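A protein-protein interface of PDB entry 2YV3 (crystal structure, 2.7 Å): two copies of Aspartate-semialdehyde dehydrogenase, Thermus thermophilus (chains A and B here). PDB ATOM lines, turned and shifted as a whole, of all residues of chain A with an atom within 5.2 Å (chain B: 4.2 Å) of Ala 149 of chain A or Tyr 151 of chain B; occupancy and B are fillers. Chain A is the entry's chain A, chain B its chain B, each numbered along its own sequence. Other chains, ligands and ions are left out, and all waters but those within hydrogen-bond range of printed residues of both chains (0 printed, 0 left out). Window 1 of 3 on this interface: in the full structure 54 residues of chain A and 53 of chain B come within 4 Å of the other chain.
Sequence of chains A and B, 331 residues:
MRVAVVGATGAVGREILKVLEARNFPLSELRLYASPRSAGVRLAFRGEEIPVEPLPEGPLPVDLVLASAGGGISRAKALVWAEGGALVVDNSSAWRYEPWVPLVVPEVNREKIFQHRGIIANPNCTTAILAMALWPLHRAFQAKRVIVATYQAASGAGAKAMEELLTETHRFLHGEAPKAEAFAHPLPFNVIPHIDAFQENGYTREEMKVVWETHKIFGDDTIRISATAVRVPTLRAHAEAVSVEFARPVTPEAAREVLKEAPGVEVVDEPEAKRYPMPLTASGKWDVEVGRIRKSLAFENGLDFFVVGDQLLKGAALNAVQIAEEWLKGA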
ATOM      1  N   ILE A 147      -1.704  34.372  23.239  1.00  0.00           N
ATOM      2  CA  ILE A 147      -0.450  33.723  22.882  1.00  0.00           C
ATOM      3  C   ILE A 147       0.291  33.256  24.127  1.00  0.00           C
ATOM      4  O   ILE A 147       1.058  34.020  24.712  1.00  0.00           O
ATOM      5  CB  ILE A 147       0.438  34.711  22.110  1.00  0.00           C
ATOM      6  CG1 ILE A 147      -0.368  35.291  20.949  1.00  0.00           C
ATOM      7  CG2 ILE A 147       1.703  34.018  21.615  1.00  0.00           C
ATOM      8  CD1 ILE A 147       0.335  36.371  20.181  1.00  0.00           C
ATOM      9  N   VAL A 148       0.090  32.010  24.534  1.00  0.00           N
ATOM     10  CA  VAL A 148       0.759  31.542  25.737  1.00  0.00           C
ATOM     11  C   VAL A 148       1.991  30.664  25.542  1.00  0.00           C
ATOM     12  O   VAL A 148       2.095  29.905  24.588  1.00  0.00           O
ATOM     13  CB  VAL A 148      -0.245  30.819  26.701  1.00  0.00           C
ATOM     14  CG1 VAL A 148      -1.632  30.707  26.043  1.00  0.00           C
ATOM     15  CG2 VAL A 148       0.279  29.438  27.090  1.00  0.00           C
ATOM     16  N   ALA A 149       2.934  30.814  26.465  1.00  0.00           N
ATOM     17  CA  ALA A 149       4.174  30.049  26.504  1.00  0.00           C
ATOM     18  C   ALA A 149       4.113  29.425  27.887  1.00  0.00           C
ATOM     19  O   ALA A 149       4.090  30.105  28.914  1.00  0.00           O
ATOM     20  CB  ALA A 149       5.377  30.948  26.386  1.00  0.00           C
ATOM     21  N   THR A 150       4.062  28.105  27.872  1.00  0.00           N
ATOM     22  CA  THR A 150       3.939  27.273  29.050  1.00  0.00           C
ATOM     23  C   THR A 150       5.280  26.868  29.626  1.00  0.00           C
ATOM     24  O   THR A 150       6.232  26.630  28.899  1.00  0.00           O
ATOM     25  CB  THR A 150       3.105  26.017  28.665  1.00  0.00           C
ATOM     26  OG1 THR A 150       1.762  26.162  29.139  1.00  0.00           O
ATOM     27  CG2 THR A 150       3.729  24.763  29.188  1.00  0.00           C
ATOM     28  N   TYR A 151       5.328  26.820  30.949  1.00  0.00           N
ATOM     29  CA  TYR A 151       6.497  26.422  31.734  1.00  0.00           C
ATOM     30  C   TYR A 151       5.912  25.284  32.587  1.00  0.00           C
ATOM     31  O   TYR A 151       5.732  25.427  33.792  1.00  0.00           O
ATOM     32  CB  TYR A 151       6.960  27.580  32.648  1.00  0.00           C
ATOM     33  CG  TYR A 151       7.468  28.825  31.924  1.00  0.00           C
ATOM     34  CD1 TYR A 151       8.830  29.109  31.851  1.00  0.00           C
ATOM     35  CD2 TYR A 151       6.594  29.674  31.267  1.00  0.00           C
ATOM     36  CE1 TYR A 151       9.296  30.198  31.131  1.00  0.00           C
ATOM     37  CE2 TYR A 151       7.048  30.762  30.550  1.00  0.00           C
ATOM     38  CZ  TYR A 151       8.389  31.024  30.475  1.00  0.00           C
ATOM     39  OH  TYR A 151       8.846  32.087  29.733  1.00  0.00           O
ATOM     40  N   VAL A 191      14.924  21.956  29.125  1.00  0.00           N
ATOM     41  CA  VAL A 191      13.515  22.147  28.858  1.00  0.00           C
ATOM     42  C   VAL A 191      13.196  21.399  27.577  1.00  0.00           C
ATOM     43  O   VAL A 191      14.028  21.336  26.672  1.00  0.00           O
ATOM     44  CB  VAL A 191      13.135  23.667  28.785  1.00  0.00           C
ATOM     45  CG1 VAL A 191      13.426  24.314  30.123  1.00  0.00           C
ATOM     46  CG2 VAL A 191      13.884  24.383  27.651  1.00  0.00           C
ATOM     47  N   THR A 228       2.633  27.420  23.213  1.00  0.00           N
ATOM     48  CA  THR A 228       3.794  26.537  23.125  1.00  0.00           C
ATOM     49  C   THR A 228       3.947  25.861  24.472  1.00  0.00           C
ATOM     50  O   THR A 228       4.363  26.503  25.428  1.00  0.00           O
ATOM     51  CB  THR A 228       5.126  27.293  22.868  1.00  0.00           C
ATOM     52  OG1 THR A 228       5.034  28.061  21.668  1.00  0.00           O
ATOM     53  CG2 THR A 228       6.300  26.278  22.738  1.00  0.00           C
ATOM     54  N   VAL A 230       5.795  23.894  27.119  1.00  0.00           N
ATOM     55  CA  VAL A 230       7.166  23.490  27.392  1.00  0.00           C
ATOM     56  C   VAL A 230       7.286  22.897  28.780  1.00  0.00           C
ATOM     57  O   VAL A 230       6.728  23.424  29.739  1.00  0.00           O
ATOM     58  CB  VAL A 230       8.145  24.643  27.220  1.00  0.00           C
ATOM     59  CG1 VAL A 230       9.587  24.118  27.368  1.00  0.00           C
ATOM     60  CG2 VAL A 230       7.933  25.288  25.852  1.00  0.00           C
ATOM     61  N   VAL A 232       9.480  21.739  32.066  1.00  0.00           N
ATOM     62  CA  VAL A 232      10.662  22.299  32.729  1.00  0.00           C
ATOM     63  C   VAL A 232      10.921  21.639  34.070  1.00  0.00           C
ATOM     64  O   VAL A 232      10.054  20.974  34.623  1.00  0.00           O
ATOM     65  CB  VAL A 232      10.540  23.815  32.959  1.00  0.00           C
ATOM     66  CG1 VAL A 232      10.195  24.512  31.644  1.00  0.00           C
ATOM     67  CG2 VAL A 232       9.491  24.103  34.046  1.00  0.00           C
ATOM     68  N   ALA A 239       3.600  27.087  35.012  1.00  0.00           N
ATOM     69  CA  ALA A 239       3.776  28.508  34.725  1.00  0.00           C
ATOM     70  C   ALA A 239       3.396  28.801  33.269  1.00  0.00           C
ATOM     71  O   ALA A 239       3.578  27.963  32.390  1.00  0.00           O
ATOM     72  CB  ALA A 239       5.207  28.910  34.969  1.00  0.00           C
ATOM     73  N   GLU A 240       2.849  29.977  33.004  1.00  0.00           N
ATOM     74  CA  GLU A 240       2.504  30.304  31.625  1.00  0.00           C
ATOM     75  C   GLU A 240       2.440  31.799  31.312  1.00  0.00           C
ATOM     76  O   GLU A 240       1.499  32.483  31.700  1.00  0.00           O
ATOM     77  CB  GLU A 240       1.187  29.612  31.215  1.00  0.00           C
ATOM     78  CG  GLU A 240       0.172  29.423  32.341  1.00  0.00           C
ATOM     79  CD  GLU A 240      -1.180  28.909  31.845  1.00  0.00           C
ATOM     80  OE1 GLU A 240      -1.850  29.626  31.061  1.00  0.00           O
ATOM     81  OE2 GLU A 240      -1.567  27.793  32.244  1.00  0.00           O
ATOM     82  N   ALA A 241       3.457  32.299  30.617  1.00  0.00           N
ATOM     83  CA  ALA A 241       3.496  33.705  30.245  1.00  0.00           C
ATOM     84  C   ALA A 241       2.383  33.922  29.238  1.00  0.00           C
ATOM     85  O   ALA A 241       2.415  33.378  28.135  1.00  0.00           O
ATOM     86  CB  ALA A 241       4.847  34.056  29.626  1.00  0.00           C
ATOM     87  N   ALA B 149       8.652  34.512  24.833  1.00  0.00           N
ATOM     88  CA  ALA B 149       8.631  34.108  26.241  1.00  0.00           C
ATOM     89  C   ALA B 149       9.918  33.341  26.486  1.00  0.00           C
ATOM     90  O   ALA B 149      10.018  32.142  26.219  1.00  0.00           O
ATOM     91  CB  ALA B 149       7.452  33.229  26.507  1.00  0.00           C
ATOM     92  N   THR B 150      10.908  34.076  26.971  1.00  0.00           N
ATOM     93  CA  THR B 150      12.239  33.571  27.269  1.00  0.00           C
ATOM     94  C   THR B 150      12.246  32.555  28.423  1.00  0.00           C
ATOM     95  O   THR B 150      11.392  32.596  29.308  1.00  0.00           O
ATOM     96  CB  THR B 150      13.192  34.793  27.600  1.00  0.00           C
ATOM     97  OG1 THR B 150      14.387  34.719  26.820  1.00  0.00           O
ATOM     98  CG2 THR B 150      13.565  34.811  29.071  1.00  0.00           C
ATOM     99  N   TYR B 151      13.219  31.646  28.356  1.00  0.00           N
ATOM    100  CA  TYR B 151      13.501  30.595  29.336  1.00  0.00           C
ATOM    101  C   TYR B 151      15.025  30.731  29.502  1.00  0.00           C
ATOM    102  O   TYR B 151      15.779  29.862  29.057  1.00  0.00           O
ATOM    103  CB  TYR B 151      13.224  29.181  28.783  1.00  0.00           C
ATOM    104  CG  TYR B 151      11.833  28.928  28.261  1.00  0.00           C
ATOM    105  CD1 TYR B 151      10.967  28.040  28.904  1.00  0.00           C
ATOM    106  CD2 TYR B 151      11.357  29.610  27.159  1.00  0.00           C
ATOM    107  CE1 TYR B 151       9.644  27.854  28.455  1.00  0.00           C
ATOM    108  CE2 TYR B 151      10.048  29.433  26.701  1.00  0.00           C
ATOM    109  CZ  TYR B 151       9.197  28.564  27.346  1.00  0.00           C
ATOM    110  OH  TYR B 151       7.907  28.430  26.877  1.00  0.00           O
ATOM    111  N   GLN B 152      15.472  31.831  30.105  1.00  0.00           N
ATOM    112  CA  GLN B 152      16.901  32.089  30.296  1.00  0.00           C
ATOM    113  C   GLN B 152      17.525  31.347  31.485  1.00  0.00           C
ATOM    114  O   GLN B 152      16.943  31.263  32.562  1.00  0.00           O
ATOM    115  CB  GLN B 152      17.150  33.601  30.438  1.00  0.00           C
ATOM    116  CG  GLN B 152      16.797  34.429  29.186  1.00  0.00           C
ATOM    117  CD  GLN B 152      16.901  35.963  29.379  1.00  0.00           C
ATOM    118  OE1 GLN B 152      17.983  36.509  29.635  1.00  0.00           O
ATOM    119  NE2 GLN B 152      15.772  36.649  29.243  1.00  0.00           N
ATOM    120  N   ALA B 153      18.736  30.842  31.286  1.00  0.00           N
ATOM    121  CA  ALA B 153      19.447  30.096  32.317  1.00  0.00           C
ATOM    122  C   ALA B 153      20.272  30.956  33.270  1.00  0.00           C
ATOM    123  O   ALA B 153      20.436  32.154  33.073  1.00  0.00           O
ATOM    124  CB  ALA B 153      20.356  29.040  31.658  1.00  0.00           C
ATOM    125  N   VAL B 230      12.100  35.006  31.837  1.00  0.00           N
ATOM    126  CA  VAL B 230      12.054  34.134  33.001  1.00  0.00           C
ATOM    127  C   VAL B 230      13.324  33.320  33.110  1.00  0.00           C
ATOM    128  O   VAL B 230      13.826  32.794  32.117  1.00  0.00           O
ATOM    129  CB  VAL B 230      10.850  33.143  32.916  1.00  0.00           C
ATOM    130  CG1 VAL B 230      10.714  32.355  34.213  1.00  0.00           C
ATOM    131  CG2 VAL B 230       9.542  33.907  32.601  1.00  0.00           C
ATOM    132  N   VAL B 232      15.078  30.069  34.337  1.00  0.00           N
ATOM    133  CA  VAL B 232      14.705  28.688  34.616  1.00  0.00           C
ATOM    134  C   VAL B 232      15.899  27.938  35.167  1.00  0.00           C
ATOM    135  O   VAL B 232      17.045  28.301  34.930  1.00  0.00           O
ATOM    136  CB  VAL B 232      14.161  27.970  33.347  1.00  0.00           C
ATOM    137  CG1 VAL B 232      13.119  28.836  32.682  1.00  0.00           C
ATOM    138  CG2 VAL B 232      15.289  27.624  32.397  1.00  0.00           C
ATOM    139  N   ALA B 237      22.205  27.376  28.726  1.00  0.00           N
ATOM    140  CA  ALA B 237      21.522  27.474  27.445  1.00  0.00           C
ATOM    141  C   ALA B 237      20.210  28.268  27.601  1.00  0.00           C
ATOM    142  O   ALA B 237      19.447  28.082  28.582  1.00  0.00           O
ATOM    143  CB  ALA B 237      21.247  26.083  26.892  1.00  0.00           C
ATOM    144  N   HIS B 238      19.971  29.158  26.636  1.00  0.00           N
ATOM    145  CA  HIS B 238      18.774  30.011  26.606  1.00  0.00           C
ATOM    146  C   HIS B 238      17.677  29.576  25.649  1.00  0.00           C
ATOM    147  O   HIS B 238      17.893  29.454  24.447  1.00  0.00           O
ATOM    148  CB  HIS B 238      19.148  31.448  26.263  1.00  0.00           C
ATOM    149  CG  HIS B 238      19.631  32.233  27.432  1.00  0.00           C
ATOM    150  ND1 HIS B 238      19.894  33.584  27.362  1.00  0.00           N
ATOM    151  CD2 HIS B 238      19.849  31.869  28.716  1.00  0.00           C
ATOM    152  CE1 HIS B 238      20.249  34.017  28.557  1.00  0.00           C
ATOM    153  NE2 HIS B 238      20.228  32.996  29.396  1.00  0.00           N
ATOM    154  N   ALA B 239      16.483  29.369  26.181  1.00  0.00           N
ATOM    155  CA  ALA B 239      15.374  28.966  25.333  1.00  0.00           C
ATOM    156  C   ALA B 239      14.368  30.097  25.170  1.00  0.00           C
ATOM    157  O   ALA B 239      14.212  30.948  26.055  1.00  0.00           O
ATOM    158  CB  ALA B 239      14.682  27.735  25.931  1.00  0.00           C
ATOM    159  N   GLU B 240      13.714  30.132  24.016  1.00  0.00           N
ATOM    160  CA  GLU B 240      12.661  31.113  23.793  1.00  0.00           C
ATOM    161  C   GLU B 240      11.632  30.552  22.840  1.00  0.00           C
ATOM    162  O   GLU B 240      11.960  29.802  21.921  1.00  0.00           O
ATOM    163  CB  GLU B 240      13.207  32.483  23.298  1.00  0.00           C
ATOM    164  CG  GLU B 240      14.380  32.463  22.353  1.00  0.00           C
ATOM    165  CD  GLU B 240      15.154  33.789  22.357  1.00  0.00           C
ATOM    166  OE1 GLU B 240      14.801  34.718  21.589  1.00  0.00           O
ATOM    167  OE2 GLU B 240      16.127  33.897  23.140  1.00  0.00           O
ATOM    168  N   ALA B 241      10.367  30.859  23.106  1.00  0.00           N
ATOM    169  CA  ALA B 241       9.278  30.414  22.243  1.00  0.00           C
ATOM    170  C   ALA B 241       8.868  31.698  21.581  1.00  0.00           C
ATOM    171  O   ALA B 241       8.621  32.685  22.266  1.00  0.00           O
ATOM    172  CB  ALA B 241       8.137  29.872  23.062  1.00  0.00           C
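The side-chain hydroxyl of Tyr 151 of chain B lies within hydrogen-bond range of the backbone carbonyl oxygen of Thr 150 of chain A, at 3.2 Å.
The side-chain hydroxyl (OH) of Tyr 151 of chain A lies within hydrogen-bond range of the backbone carbonyl oxygen (O) of Thr 150 of chain B, at 2.6 Å.
The backbone NH (N) of Ala 241 of chain A sits at hydrogen-bond distance from the backbone carbonyl oxygen (O) of Ala 149 of chain A.
N of Thr 150 of chain A is in hydrogen-bond range of O of Thr 228 of chain A, at 2.9 Å.
N of Tyr 151 of chain A is in hydrogen-bond range of O of Ala 239 of chain A, at 2.5 Å.
The side-chain amide nitrogen (NE2) of Gln 152 of chain B lies close to the side-chain hydroxyl (OG1) of Thr 150 of chain B (3.4 Å).
The backbone NH (N) of Tyr 151 of chain B sits at hydrogen-bond distance from the backbone carbonyl oxygen (O) of Ala 239 of chain B, 2.6 Å away.
N of Gln 152 of chain B sits at hydrogen-bond distance from O of Val 230 of chain B (2.8 Å).
CB of Ala 149 of chain A touches CB of Ala 149 of chain B (3.1 Å).
Tyr 151 of chain B touches Ala 149 of chain A (OH to CB, 3.6 Å).
C of Ala 149 of chain B touches OH of Tyr 151 of chain A, 3.6 Å away.
Tyr 151 of chain B touches Tyr 151 of chain A (CD1 to CE1, 3.5 Å).
OH of Tyr 151 of chain A touches CG2 of Val 230 of chain B (3.5 Å).
Val 191 of chain A touches Ala 239 of chain B (CG2 to CB, 3.9 Å).
CB of Ala 241 of chain B touches OG1 of Thr 228 of chain A, at 3.9 Å.
Tyr 151 of chain B touches Val 230 of chain A.
Of chain B, only Ala 149 and Tyr 151 come within 4 Å of Ala 149 of chain A.
Of the printed residues of chain B, Val 191 of chain A touches Ala 239 (3.9 Å).
Printed residues of chain B within 4 Å of Val 230 of chain A: Tyr 151.
Of chain A, only Ala 149 (3.6 Å), Thr 150 (3.2 Å), Tyr 151 (3.5 Å) and Val 230 (3.3 Å) come within 4 Å of Tyr 151 of chain B.
Printed residues of chain A that touch a printed residue of chain B: Ala 149, Thr 150, Tyr 151, Val 191, Thr 228 and Val 230.
Hydrophobic or aromatic side chains of chain A within 4 Å of the printed part of chain B: Ala 149, Tyr 151, Val 191 and Val 230.
Along chain A the printed residues that touch a printed residue of chain B span positions 149 to 230.
Hydrophobic or aromatic side chains of chain B that line the printed part of chain A: Ala 149, Tyr 151, Val 230, Ala 239 and Ala 241.
Ala 149 of chain B touches its own counterpart, Ala 149 of chain A.
Ala 149 of chain A touches Tyr 151 of chain B, and with the chains exchanged Tyr 151 of chain A touches Ala 149 of chain B.
Thr 150 of chain A touches Tyr 151 of chain B, and with the chains exchanged Tyr 151 of chain A touches Thr 150 of chain B.
Tyr 151 of chain B touches its own counterpart, Tyr 151 of chain A.
Positions printed for both chains: 149, 150, 151, 230, 232, 239, 240 and 241.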
